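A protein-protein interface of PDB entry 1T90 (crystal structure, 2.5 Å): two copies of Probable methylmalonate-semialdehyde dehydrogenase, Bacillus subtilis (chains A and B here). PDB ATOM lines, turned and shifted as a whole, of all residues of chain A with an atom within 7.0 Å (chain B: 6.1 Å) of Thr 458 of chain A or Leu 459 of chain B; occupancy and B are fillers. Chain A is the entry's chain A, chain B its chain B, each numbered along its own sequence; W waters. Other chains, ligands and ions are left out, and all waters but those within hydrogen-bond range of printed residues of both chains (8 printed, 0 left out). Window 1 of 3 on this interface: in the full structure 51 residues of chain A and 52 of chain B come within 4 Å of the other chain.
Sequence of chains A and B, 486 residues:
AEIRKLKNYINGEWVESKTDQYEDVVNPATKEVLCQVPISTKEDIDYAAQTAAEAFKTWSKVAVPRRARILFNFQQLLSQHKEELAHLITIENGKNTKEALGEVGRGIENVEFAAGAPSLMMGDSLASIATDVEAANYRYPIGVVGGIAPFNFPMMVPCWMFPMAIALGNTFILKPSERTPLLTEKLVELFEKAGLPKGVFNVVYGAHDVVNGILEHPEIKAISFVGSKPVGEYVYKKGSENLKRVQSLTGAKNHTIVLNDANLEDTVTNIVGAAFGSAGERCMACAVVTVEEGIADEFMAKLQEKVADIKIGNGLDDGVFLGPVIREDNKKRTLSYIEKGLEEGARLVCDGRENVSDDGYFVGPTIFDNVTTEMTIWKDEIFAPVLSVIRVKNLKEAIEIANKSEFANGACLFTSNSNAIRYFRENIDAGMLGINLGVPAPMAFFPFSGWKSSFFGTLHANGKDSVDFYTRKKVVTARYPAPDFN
OD2 of Asp 465 of chain B lies within salt-bridge range of NZ of Lys 473 of chain A.
The backbone carbonyl oxygen of Asp 468 of chain A sits at hydrogen-bond distance from the guanidinium group of Arg 245 of chain A (3.3 Å).
The guanidinium group of Arg 245 of chain A sits at hydrogen-bond distance from the backbone carbonyl oxygen of Phe 469 of chain A (2.8 Å).
The side-chain carboxylate (OD1) of Asp 465 of chain B lies within hydrogen-bond range of the backbone NH (N) of His 460 of chain B, at 3.1 Å.
The side-chain amide nitrogen (NE2) of Gln 247 of chain B is in hydrogen-bond range of the backbone carbonyl oxygen (O) of Leu 459 of chain B (2.8 Å).
Arg 245 of chain A touches Gly 457 of chain B.
Arg 245 of chain A touches Thr 458 of chain B.
CZ3 of Trp 451 of chain A touches NH2 of Arg 245 of chain B, 3.7 Å away.
Gly 457 of chain A touches Arg 245 of chain B (O to NH2, 3.9 Å).
Thr 458 of chain A touches Arg 245 of chain B (OG1 to CB, 3.7 Å).
Leu 459 of chain B touches Thr 458 of chain A (CD1 to CG2, 3.7 Å).
Leu 459 of chain A touches Thr 458 of chain B (CD1 to CG2, 3.5 Å).
Printed residues of chain B within 4 Å of Thr 458 of chain A: Arg 245 and Leu 459.
Leu 459 of chain B touches just one residue of chain A: Thr 458 (3.7 Å).
Of the printed residues of chain B, Trp 451 of chain A touches Arg 245.
Printed residues of chain B within 4 Å of Arg 245 of chain A: Gly 457 and Thr 458.
Printed residues of chain A within 4 Å of Thr 458 of chain B: Arg 245 (3.8 Å) and Leu 459 (3.5 Å).
Lys 464 of chain B touches none of the printed residues of chain A.
The nearest residue of chain B that does not touch Thr 458 of chain A is Phe 469 of chain B (4.04 Å).
Hydrophobic or aromatic side chains of chain A within 4 Å of the printed part of chain B: Trp 451 and Leu 459.
Of the 18 printed residues of chain B, 5 touch a printed residue of chain A.
Hydrophobic or aromatic side chains of chain B within 4 Å of the printed part of chain A: Leu 459.
Among the printed residues, Asp or Glu carboxylates within 4 Å of a Lys or Arg side-chain nitrogen of the other chain: Lys 473 of chain A with Asp 465 of chain B.
Arg 245 of chain A touches Gly 457 of chain B, and with the chains exchanged Gly 457 of chain A touches Arg 245 of chain B.
Arg 245 of chain A touches Thr 458 of chain B, and with the chains exchanged Thr 458 of chain A touches Arg 245 of chain B.
Thr 458 of chain A touches Leu 459 of chain B, and with the chains exchanged Leu 459 of chain A touches Thr 458 of chain B.
Positions printed for both chains: 245, 246, 247, 455, 456, 457, 458, 459, 460, 465, 468 and 469.
Of the 8 pairs that touch across the chains among the printed residues, 6 have their exchanged pair printed and touching as well.
Water W2 lies within hydrogen-bond range of the side-chain hydroxyl (OG1) of Thr 458 of chain A, the backbone NH (N) of Thr 458 of chain B and the backbone NH (N) of Leu 459 of chain B.
Water W5 bridges the side-chain carboxylate of Asp 465 of chain B (2.6 Å) and the side-chain amino group of Lys 473 of chain A (2.8 Å).
Water W7 bridges NH2 of Arg 245 of chain A and O of Thr 458 of chain B.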
ATOM      1  N   TYR A 236      31.148   6.230  -8.682  1.00  0.00           N
ATOM      2  CA  TYR A 236      30.033   6.340  -9.614  1.00  0.00           C
ATOM      3  C   TYR A 236      29.052   5.201  -9.385  1.00  0.00           C
ATOM      4  O   TYR A 236      27.848   5.410  -9.258  1.00  0.00           O
ATOM      5  CB  TYR A 236      30.520   6.269 -11.058  1.00  0.00           C
ATOM      6  CG  TYR A 236      29.430   6.617 -12.034  1.00  0.00           C
ATOM      7  CD1 TYR A 236      29.132   7.950 -12.325  1.00  0.00           C
ATOM      8  CD2 TYR A 236      28.628   5.624 -12.596  1.00  0.00           C
ATOM      9  CE1 TYR A 236      28.062   8.286 -13.141  1.00  0.00           C
ATOM     10  CE2 TYR A 236      27.549   5.948 -13.415  1.00  0.00           C
ATOM     11  CZ  TYR A 236      27.269   7.283 -13.680  1.00  0.00           C
ATOM     12  OH  TYR A 236      26.185   7.619 -14.461  1.00  0.00           O
ATOM     13  N   ARG A 245      22.663  11.294  -8.155  1.00  0.00           N
ATOM     14  CA  ARG A 245      23.396  11.677  -9.345  1.00  0.00           C
ATOM     15  C   ARG A 245      24.849  11.834  -8.966  1.00  0.00           C
ATOM     16  O   ARG A 245      25.166  12.257  -7.853  1.00  0.00           O
ATOM     17  CB  ARG A 245      22.860  12.995  -9.927  1.00  0.00           C
ATOM     18  CG  ARG A 245      23.094  14.234  -9.075  1.00  0.00           C
ATOM     19  CD  ARG A 245      22.547  15.480  -9.763  1.00  0.00           C
ATOM     20  NE  ARG A 245      21.106  15.393  -9.985  1.00  0.00           N
ATOM     21  CZ  ARG A 245      20.373  16.340 -10.563  1.00  0.00           C
ATOM     22  NH1 ARG A 245      20.942  17.460 -10.980  1.00  0.00           N
ATOM     23  NH2 ARG A 245      19.068  16.164 -10.733  1.00  0.00           N
ATOM     24  N   VAL A 246      25.732  11.491  -9.895  1.00  0.00           N
ATOM     25  CA  VAL A 246      27.158  11.603  -9.650  1.00  0.00           C
ATOM     26  C   VAL A 246      27.958  11.863 -10.920  1.00  0.00           C
ATOM     27  O   VAL A 246      27.551  11.497 -12.024  1.00  0.00           O
ATOM     28  CB  VAL A 246      27.691  10.328  -8.906  1.00  0.00           C
ATOM     29  CG1 VAL A 246      26.886   9.125  -9.302  1.00  0.00           C
ATOM     30  CG2 VAL A 246      29.165  10.101  -9.202  1.00  0.00           C
ATOM     31  N   GLN A 247      29.086  12.541 -10.749  1.00  0.00           N
ATOM     32  CA  GLN A 247      29.976  12.841 -11.852  1.00  0.00           C
ATOM     33  C   GLN A 247      31.398  12.518 -11.403  1.00  0.00           C
ATOM     34  O   GLN A 247      31.888  13.056 -10.405  1.00  0.00           O
ATOM     35  CB  GLN A 247      29.859  14.315 -12.262  1.00  0.00           C
ATOM     36  CG  GLN A 247      30.070  15.311 -11.130  1.00  0.00           C
ATOM     37  CD  GLN A 247      29.944  16.757 -11.585  1.00  0.00           C
ATOM     38  OE1 GLN A 247      30.108  17.674 -10.797  1.00  0.00           O
ATOM     39  NE2 GLN A 247      29.650  16.958 -12.858  1.00  0.00           N
ATOM     40  N   TRP A 451      36.110  12.086 -21.625  1.00  0.00           N
ATOM     41  CA  TRP A 451      35.380  10.973 -22.236  1.00  0.00           C
ATOM     42  C   TRP A 451      35.973   9.590 -21.905  1.00  0.00           C
ATOM     43  O   TRP A 451      37.086   9.481 -21.374  1.00  0.00           O
ATOM     44  CB  TRP A 451      35.345  11.182 -23.757  1.00  0.00           C
ATOM     45  CG  TRP A 451      34.231  10.485 -24.475  1.00  0.00           C
ATOM     46  CD1 TRP A 451      34.348   9.652 -25.553  1.00  0.00           C
ATOM     47  CD2 TRP A 451      32.829  10.572 -24.185  1.00  0.00           C
ATOM     48  NE1 TRP A 451      33.109   9.214 -25.950  1.00  0.00           N
ATOM     49  CE2 TRP A 451      32.158   9.760 -25.130  1.00  0.00           C
ATOM     50  CE3 TRP A 451      32.076  11.255 -23.221  1.00  0.00           C
ATOM     51  CZ2 TRP A 451      30.766   9.608 -25.138  1.00  0.00           C
ATOM     52  CZ3 TRP A 451      30.697  11.107 -23.227  1.00  0.00           C
ATOM     53  CH2 TRP A 451      30.054  10.284 -24.183  1.00  0.00           C
ATOM     54  N   PHE A 455      35.791   9.935 -17.883  1.00  0.00           N
ATOM     55  CA  PHE A 455      34.573  10.554 -17.372  1.00  0.00           C
ATOM     56  C   PHE A 455      33.384   9.608 -17.237  1.00  0.00           C
ATOM     57  O   PHE A 455      32.958   8.976 -18.209  1.00  0.00           O
ATOM     58  CB  PHE A 455      34.146  11.721 -18.263  1.00  0.00           C
ATOM     59  CG  PHE A 455      32.816  12.302 -17.883  1.00  0.00           C
ATOM     60  CD1 PHE A 455      32.662  12.994 -16.682  1.00  0.00           C
ATOM     61  CD2 PHE A 455      31.711  12.127 -18.699  1.00  0.00           C
ATOM     62  CE1 PHE A 455      31.415  13.502 -16.300  1.00  0.00           C
ATOM     63  CE2 PHE A 455      30.465  12.629 -18.329  1.00  0.00           C
ATOM     64  CZ  PHE A 455      30.318  13.319 -17.125  1.00  0.00           C
ATOM     65  N   PHE A 456      32.833   9.534 -16.032  1.00  0.00           N
ATOM     66  CA  PHE A 456      31.675   8.689 -15.784  1.00  0.00           C
ATOM     67  C   PHE A 456      30.498   9.567 -15.389  1.00  0.00           C
ATOM     68  O   PHE A 456      30.516  10.199 -14.332  1.00  0.00           O
ATOM     69  CB  PHE A 456      31.972   7.681 -14.666  1.00  0.00           C
ATOM     70  CG  PHE A 456      33.106   6.761 -14.980  1.00  0.00           C
ATOM     71  CD1 PHE A 456      34.238   6.732 -14.173  1.00  0.00           C
ATOM     72  CD2 PHE A 456      33.062   5.948 -16.110  1.00  0.00           C
ATOM     73  CE1 PHE A 456      35.320   5.906 -14.488  1.00  0.00           C
ATOM     74  CE2 PHE A 456      34.134   5.120 -16.437  1.00  0.00           C
ATOM     75  CZ  PHE A 456      35.267   5.098 -15.624  1.00  0.00           C
ATOM     76  N   GLY A 457      29.484   9.607 -16.246  1.00  0.00           N
ATOM     77  CA  GLY A 457      28.301  10.405 -15.967  1.00  0.00           C
ATOM     78  C   GLY A 457      27.706  11.052 -17.205  1.00  0.00           C
ATOM     79  O   GLY A 457      27.975  10.619 -18.330  1.00  0.00           O
ATOM     80  N   THR A 458      26.894  12.087 -17.000  1.00  0.00           N
ATOM     81  CA  THR A 458      26.270  12.804 -18.108  1.00  0.00           C
ATOM     82  C   THR A 458      26.819  14.223 -18.200  1.00  0.00           C
ATOM     83  O   THR A 458      27.335  14.642 -19.235  1.00  0.00           O
ATOM     84  CB  THR A 458      24.745  12.884 -17.935  1.00  0.00           C
ATOM     85  OG1 THR A 458      24.225  11.576 -17.681  1.00  0.00           O
ATOM     86  CG2 THR A 458      24.098  13.427 -19.199  1.00  0.00           C
ATOM     87  N   LEU A 459      26.715  14.957 -17.104  1.00  0.00           N
ATOM     88  CA  LEU A 459      27.192  16.330 -17.054  1.00  0.00           C
ATOM     89  C   LEU A 459      28.595  16.436 -16.467  1.00  0.00           C
ATOM     90  O   LEU A 459      28.893  15.843 -15.440  1.00  0.00           O
ATOM     91  CB  LEU A 459      26.218  17.177 -16.236  1.00  0.00           C
ATOM     92  CG  LEU A 459      24.818  17.287 -16.844  1.00  0.00           C
ATOM     93  CD1 LEU A 459      23.921  18.103 -15.930  1.00  0.00           C
ATOM     94  CD2 LEU A 459      24.915  17.930 -18.229  1.00  0.00           C
ATOM     95  N   HIS A 460      29.450  17.204 -17.131  1.00  0.00           N
ATOM     96  CA  HIS A 460      30.821  17.396 -16.679  1.00  0.00           C
ATOM     97  C   HIS A 460      30.855  18.450 -15.584  1.00  0.00           C
ATOM     98  O   HIS A 460      29.813  18.903 -15.113  1.00  0.00           O
ATOM     99  CB  HIS A 460      31.702  17.873 -17.836  1.00  0.00           C
ATOM    100  CG  HIS A 460      31.714  16.948 -19.013  1.00  0.00           C
ATOM    101  ND1 HIS A 460      32.304  15.701 -18.975  1.00  0.00           N
ATOM    102  CD2 HIS A 460      31.216  17.092 -20.263  1.00  0.00           C
ATOM    103  CE1 HIS A 460      32.169  15.119 -20.154  1.00  0.00           C
ATOM    104  NE2 HIS A 460      31.513  15.942 -20.953  1.00  0.00           N
ATOM    105  N   ASP A 465      27.258  22.915 -17.755  1.00  0.00           N
ATOM    106  CA  ASP A 465      27.037  21.538 -17.327  1.00  0.00           C
ATOM    107  C   ASP A 465      26.951  21.486 -15.807  1.00  0.00           C
ATOM    108  O   ASP A 465      26.113  20.769 -15.248  1.00  0.00           O
ATOM    109  CB  ASP A 465      28.175  20.620 -17.790  1.00  0.00           C
ATOM    110  CG  ASP A 465      27.946  20.051 -19.181  1.00  0.00           C
ATOM    111  OD1 ASP A 465      28.717  19.158 -19.584  1.00  0.00           O
ATOM    112  OD2 ASP A 465      27.003  20.492 -19.876  1.00  0.00           O
ATOM    113  N   ASP A 468      23.436  22.680 -14.433  1.00  0.00           N
ATOM    114  CA  ASP A 468      22.367  21.688 -14.481  1.00  0.00           C
ATOM    115  C   ASP A 468      22.641  20.494 -13.578  1.00  0.00           C
ATOM    116  O   ASP A 468      21.708  19.877 -13.069  1.00  0.00           O
ATOM    117  CB  ASP A 468      22.153  21.210 -15.918  1.00  0.00           C
ATOM    118  CG  ASP A 468      21.439  22.240 -16.774  1.00  0.00           C
ATOM    119  OD1 ASP A 468      21.882  23.404 -16.810  1.00  0.00           O
ATOM    120  OD2 ASP A 468      20.430  21.893 -17.420  1.00  0.00           O
ATOM    121  N   PHE A 469      23.914  20.165 -13.381  1.00  0.00           N
ATOM    122  CA  PHE A 469      24.258  19.040 -12.519  1.00  0.00           C
ATOM    123  C   PHE A 469      23.910  19.358 -11.068  1.00  0.00           C
ATOM    124  O   PHE A 469      23.425  18.495 -10.337  1.00  0.00           O
ATOM    125  CB  PHE A 469      25.751  18.714 -12.617  1.00  0.00           C
ATOM    126  CG  PHE A 469      26.187  17.626 -11.678  1.00  0.00           C
ATOM    127  CD1 PHE A 469      25.868  16.294 -11.935  1.00  0.00           C
ATOM    128  CD2 PHE A 469      26.862  17.935 -10.498  1.00  0.00           C
ATOM    129  CE1 PHE A 469      26.212  15.282 -11.019  1.00  0.00           C
ATOM    130  CE2 PHE A 469      27.205  16.939  -9.583  1.00  0.00           C
ATOM    131  CZ  PHE A 469      26.878  15.612  -9.845  1.00  0.00           C
ATOM    132  N   LYS A 473      14.905  21.045 -12.143  1.00  0.00           N
ATOM    133  CA  LYS A 473      13.872  21.936 -12.644  1.00  0.00           C
ATOM    134  C   LYS A 473      12.441  21.621 -12.260  1.00  0.00           C
ATOM    135  O   LYS A 473      12.085  20.481 -11.985  1.00  0.00           O
ATOM    136  CB  LYS A 473      13.953  22.017 -14.171  1.00  0.00           C
ATOM    137  CG  LYS A 473      15.320  22.396 -14.711  1.00  0.00           C
ATOM    138  CD  LYS A 473      15.340  22.362 -16.234  1.00  0.00           C
ATOM    139  CE  LYS A 473      16.739  22.601 -16.780  1.00  0.00           C
ATOM    140  NZ  LYS A 473      17.630  21.436 -16.513  1.00  0.00           N
ATOM    141  N   ARG B 245      25.354   6.130 -19.339  1.00  0.00           N
ATOM    142  CA  ARG B 245      24.389   7.102 -18.867  1.00  0.00           C
ATOM    143  C   ARG B 245      22.997   6.531 -19.067  1.00  0.00           C
ATOM    144  O   ARG B 245      22.711   5.893 -20.089  1.00  0.00           O
ATOM    145  CB  ARG B 245      24.528   8.416 -19.631  1.00  0.00           C
ATOM    146  CG  ARG B 245      24.228   8.311 -21.109  1.00  0.00           C
ATOM    147  CD  ARG B 245      24.303   9.677 -21.753  1.00  0.00           C
ATOM    148  NE  ARG B 245      25.654  10.226 -21.665  1.00  0.00           N
ATOM    149  CZ  ARG B 245      26.005  11.429 -22.108  1.00  0.00           C
ATOM    150  NH1 ARG B 245      25.102  12.222 -22.673  1.00  0.00           N
ATOM    151  NH2 ARG B 245      27.264  11.832 -21.995  1.00  0.00           N
ATOM    152  N   VAL B 246      22.136   6.752 -18.080  1.00  0.00           N
ATOM    153  CA  VAL B 246      20.772   6.265 -18.156  1.00  0.00           C
ATOM    154  C   VAL B 246      19.821   7.269 -17.524  1.00  0.00           C
ATOM    155  O   VAL B 246      20.221   8.062 -16.674  1.00  0.00           O
ATOM    156  CB  VAL B 246      20.645   4.855 -17.483  1.00  0.00           C
ATOM    157  CG1 VAL B 246      21.792   4.634 -16.524  1.00  0.00           C
ATOM    158  CG2 VAL B 246      19.298   4.707 -16.767  1.00  0.00           C
ATOM    159  N   GLN B 247      18.573   7.268 -17.980  1.00  0.00           N
ATOM    160  CA  GLN B 247      17.566   8.163 -17.432  1.00  0.00           C
ATOM    161  C   GLN B 247      16.309   7.331 -17.270  1.00  0.00           C
ATOM    162  O   GLN B 247      15.816   6.725 -18.231  1.00  0.00           O
ATOM    163  CB  GLN B 247      17.323   9.357 -18.363  1.00  0.00           C
ATOM    164  CG  GLN B 247      16.718   9.008 -19.707  1.00  0.00           C
ATOM    165  CD  GLN B 247      16.562  10.218 -20.614  1.00  0.00           C
ATOM    166  OE1 GLN B 247      16.076  10.102 -21.734  1.00  0.00           O
ATOM    167  NE2 GLN B 247      16.980  11.385 -20.132  1.00  0.00           N
ATOM    168  N   SER B 248      15.804   7.278 -16.044  1.00  0.00           N
ATOM    169  CA  SER B 248      14.618   6.489 -15.771  1.00  0.00           C
ATOM    170  C   SER B 248      13.456   7.318 -15.281  1.00  0.00           C
ATOM    171  O   SER B 248      13.492   7.845 -14.166  1.00  0.00           O
ATOM    172  CB  SER B 248      14.910   5.419 -14.716  1.00  0.00           C
ATOM    173  OG  SER B 248      15.742   4.398 -15.211  1.00  0.00           O
ATOM    174  N   LEU B 249      12.427   7.432 -16.112  1.00  0.00           N
ATOM    175  CA  LEU B 249      11.223   8.156 -15.737  1.00  0.00           C
ATOM    176  C   LEU B 249      10.274   7.063 -15.231  1.00  0.00           C
ATOM    177  O   LEU B 249       9.788   6.228 -16.003  1.00  0.00           O
ATOM    178  CB  LEU B 249      10.660   8.896 -16.948  1.00  0.00           C
ATOM    179  CG  LEU B 249      11.462  10.141 -17.355  1.00  0.00           C
ATOM    180  CD1 LEU B 249      12.869   9.755 -17.806  1.00  0.00           C
ATOM    181  CD2 LEU B 249      10.721  10.876 -18.465  1.00  0.00           C
ATOM    182  N   PHE B 455      11.861   9.939 -10.818  1.00  0.00           N
ATOM    183  CA  PHE B 455      12.938  10.157 -11.760  1.00  0.00           C
ATOM    184  C   PHE B 455      14.275   9.685 -11.203  1.00  0.00           C
ATOM    185  O   PHE B 455      14.589   9.906 -10.034  1.00  0.00           O
ATOM    186  CB  PHE B 455      13.039  11.642 -12.129  1.00  0.00           C
ATOM    187  CG  PHE B 455      14.240  11.965 -12.971  1.00  0.00           C
ATOM    188  CD1 PHE B 455      14.382  11.413 -14.240  1.00  0.00           C
ATOM    189  CD2 PHE B 455      15.251  12.778 -12.481  1.00  0.00           C
ATOM    190  CE1 PHE B 455      15.512  11.664 -15.004  1.00  0.00           C
ATOM    191  CE2 PHE B 455      16.383  13.038 -13.235  1.00  0.00           C
ATOM    192  CZ  PHE B 455      16.513  12.479 -14.499  1.00  0.00           C
ATOM    193  N   PHE B 456      15.058   9.037 -12.058  1.00  0.00           N
ATOM    194  CA  PHE B 456      16.376   8.544 -11.691  1.00  0.00           C
ATOM    195  C   PHE B 456      17.362   9.011 -12.755  1.00  0.00           C
ATOM    196  O   PHE B 456      17.260   8.630 -13.925  1.00  0.00           O
ATOM    197  CB  PHE B 456      16.368   7.009 -11.600  1.00  0.00           C
ATOM    198  CG  PHE B 456      15.556   6.474 -10.446  1.00  0.00           C
ATOM    199  CD1 PHE B 456      14.608   5.468 -10.648  1.00  0.00           C
ATOM    200  CD2 PHE B 456      15.728   6.985  -9.157  1.00  0.00           C
ATOM    201  CE1 PHE B 456      13.836   4.977  -9.583  1.00  0.00           C
ATOM    202  CE2 PHE B 456      14.966   6.504  -8.086  1.00  0.00           C
ATOM    203  CZ  PHE B 456      14.014   5.496  -8.300  1.00  0.00           C
ATOM    204  N   GLY B 457      18.306   9.850 -12.349  1.00  0.00           N
ATOM    205  CA  GLY B 457      19.282  10.348 -13.293  1.00  0.00           C
ATOM    206  C   GLY B 457      19.518  11.835 -13.148  1.00  0.00           C
ATOM    207  O   GLY B 457      19.254  12.422 -12.098  1.00  0.00           O
ATOM    208  N   THR B 458      20.016  12.462 -14.204  1.00  0.00           N
ATOM    209  CA  THR B 458      20.282  13.888 -14.133  1.00  0.00           C
ATOM    210  C   THR B 458      19.395  14.646 -15.090  1.00  0.00           C
ATOM    211  O   THR B 458      18.737  15.607 -14.708  1.00  0.00           O
ATOM    212  CB  THR B 458      21.741  14.205 -14.482  1.00  0.00           C
ATOM    213  OG1 THR B 458      22.612  13.405 -13.671  1.00  0.00           O
ATOM    214  CG2 THR B 458      22.029  15.687 -14.244  1.00  0.00           C
ATOM    215  N   LEU B 459      19.383  14.207 -16.341  1.00  0.00           N
ATOM    216  CA  LEU B 459      18.578  14.862 -17.352  1.00  0.00           C
ATOM    217  C   LEU B 459      17.306  14.081 -17.666  1.00  0.00           C
ATOM    218  O   LEU B 459      17.323  12.855 -17.768  1.00  0.00           O
ATOM    219  CB  LEU B 459      19.425  15.069 -18.605  1.00  0.00           C
ATOM    220  CG  LEU B 459      20.660  15.928 -18.315  1.00  0.00           C
ATOM    221  CD1 LEU B 459      21.526  16.051 -19.557  1.00  0.00           C
ATOM    222  CD2 LEU B 459      20.216  17.307 -17.842  1.00  0.00           C
ATOM    223  N   HIS B 460      16.199  14.801 -17.810  1.00  0.00           N
ATOM    224  CA  HIS B 460      14.915  14.176 -18.095  1.00  0.00           C
ATOM    225  C   HIS B 460      14.714  13.975 -19.589  1.00  0.00           C
ATOM    226  O   HIS B 460      15.618  14.196 -20.400  1.00  0.00           O
ATOM    227  CB  HIS B 460      13.766  15.051 -17.584  1.00  0.00           C
ATOM    228  CG  HIS B 460      13.905  15.468 -16.157  1.00  0.00           C
ATOM    229  ND1 HIS B 460      13.694  14.605 -15.104  1.00  0.00           N
ATOM    230  CD2 HIS B 460      14.251  16.657 -15.610  1.00  0.00           C
ATOM    231  CE1 HIS B 460      13.903  15.247 -13.969  1.00  0.00           C
ATOM    232  NE2 HIS B 460      14.243  16.492 -14.248  1.00  0.00           N
ATOM    233  N   ALA B 461      13.501  13.562 -19.938  1.00  0.00           N
ATOM    234  CA  ALA B 461      13.146  13.371 -21.328  1.00  0.00           C
ATOM    235  C   ALA B 461      12.656  14.722 -21.831  1.00  0.00           C
ATOM    236  O   ALA B 461      12.228  15.574 -21.034  1.00  0.00           O
ATOM    237  CB  ALA B 461      12.037  12.331 -21.455  1.00  0.00           C
ATOM    238  N   LYS B 464      15.484  20.739 -23.636  1.00  0.00           N
ATOM    239  CA  LYS B 464      16.905  20.795 -23.923  1.00  0.00           C
ATOM    240  C   LYS B 464      17.606  19.695 -23.133  1.00  0.00           C
ATOM    241  O   LYS B 464      18.747  19.340 -23.414  1.00  0.00           O
ATOM    242  CB  LYS B 464      17.450  22.174 -23.563  1.00  0.00           C
ATOM    243  CG  LYS B 464      16.624  23.313 -24.167  1.00  0.00           C
ATOM    244  CD  LYS B 464      17.116  24.672 -23.697  1.00  0.00           C
ATOM    245  CE  LYS B 464      15.980  25.681 -23.599  1.00  0.00           C
ATOM    246  NZ  LYS B 464      15.425  26.027 -24.926  1.00  0.00           N
ATOM    247  N   ASP B 465      16.910  19.142 -22.144  1.00  0.00           N
ATOM    248  CA  ASP B 465      17.487  18.071 -21.355  1.00  0.00           C
ATOM    249  C   ASP B 465      17.778  16.890 -22.268  1.00  0.00           C
ATOM    250  O   ASP B 465      18.883  16.343 -22.242  1.00  0.00           O
ATOM    251  CB  ASP B 465      16.542  17.621 -20.239  1.00  0.00           C
ATOM    252  CG  ASP B 465      16.731  18.404 -18.953  1.00  0.00           C
ATOM    253  OD1 ASP B 465      16.293  17.901 -17.897  1.00  0.00           O
ATOM    254  OD2 ASP B 465      17.304  19.514 -18.993  1.00  0.00           O
ATOM    255  N   SER B 466      16.793  16.506 -23.078  1.00  0.00           N
ATOM    256  CA  SER B 466      16.978  15.383 -23.976  1.00  0.00           C
ATOM    257  C   SER B 466      18.143  15.644 -24.920  1.00  0.00           C
ATOM    258  O   SER B 466      18.871  14.722 -25.277  1.00  0.00           O
ATOM    259  CB  SER B 466      15.689  15.089 -24.764  1.00  0.00           C
ATOM    260  OG  SER B 466      15.343  16.131 -25.659  1.00  0.00           O
ATOM    261  N   ASP B 468      20.988  17.341 -24.338  1.00  0.00           N
ATOM    262  CA  ASP B 468      22.250  17.100 -23.650  1.00  0.00           C
ATOM    263  C   ASP B 468      22.443  15.633 -23.310  1.00  0.00           C
ATOM    264  O   ASP B 468      23.563  15.128 -23.303  1.00  0.00           O
ATOM    265  CB  ASP B 468      22.324  17.912 -22.357  1.00  0.00           C
ATOM    266  CG  ASP B 468      22.638  19.362 -22.605  1.00  0.00           C
ATOM    267  OD1 ASP B 468      23.521  19.624 -23.445  1.00  0.00           O
ATOM    268  OD2 ASP B 468      22.017  20.233 -21.953  1.00  0.00           O
ATOM    269  N   PHE B 469      21.346  14.945 -23.028  1.00  0.00           N
ATOM    270  CA  PHE B 469      21.440  13.550 -22.680  1.00  0.00           C
ATOM    271  C   PHE B 469      21.854  12.689 -23.869  1.00  0.00           C
ATOM    272  O   PHE B 469      22.530  11.671 -23.703  1.00  0.00           O
ATOM    273  CB  PHE B 469      20.110  13.052 -22.135  1.00  0.00           C
ATOM    274  CG  PHE B 469      20.172  11.651 -21.620  1.00  0.00           C
ATOM    275  CD1 PHE B 469      20.844  11.366 -20.429  1.00  0.00           C
ATOM    276  CD2 PHE B 469      19.605  10.605 -22.347  1.00  0.00           C
ATOM    277  CE1 PHE B 469      20.951  10.052 -19.964  1.00  0.00           C
ATOM    278  CE2 PHE B 469      19.705   9.287 -21.895  1.00  0.00           C
ATOM    279  CZ  PHE B 469      20.383   9.011 -20.698  1.00  0.00           C
ATOM    280  N   THR B 471      23.806  13.659 -26.389  1.00  0.00           N
ATOM    281  CA  THR B 471      25.006  14.163 -27.038  1.00  0.00           C
ATOM    282  C   THR B 471      26.128  14.285 -26.026  1.00  0.00           C
ATOM    283  O   THR B 471      25.915  14.096 -24.828  1.00  0.00           O
ATOM    284  CB  THR B 471      24.768  15.558 -27.651  1.00  0.00           C
ATOM    285  OG1 THR B 471      24.450  16.489 -26.609  1.00  0.00           O
ATOM    286  CG2 THR B 471      23.621  15.511 -28.655  1.00  0.00           C
HETATM  287  O   HOH W   1      15.247  18.653 -13.221  1.00  0.00           O
HETATM  288  O   HOH W   2      22.008  11.934 -16.454  1.00  0.00           O
HETATM  289  O   HOH W   3      18.662  13.645  -9.538  1.00  0.00           O
HETATM  290  O   HOH W   4      28.540   9.020 -20.538  1.00  0.00           O
HETATM  291  O   HOH W   5      16.694  18.948 -15.535  1.00  0.00           O
HETATM  292  O   HOH W   6      27.881  14.449 -21.957  1.00  0.00           O
HETATM  293  O   HOH W   7      17.792  17.457 -12.794  1.00  0.00           O
HETATM  294  O   HOH W   8      18.652  21.771 -19.980  1.00  0.00           O
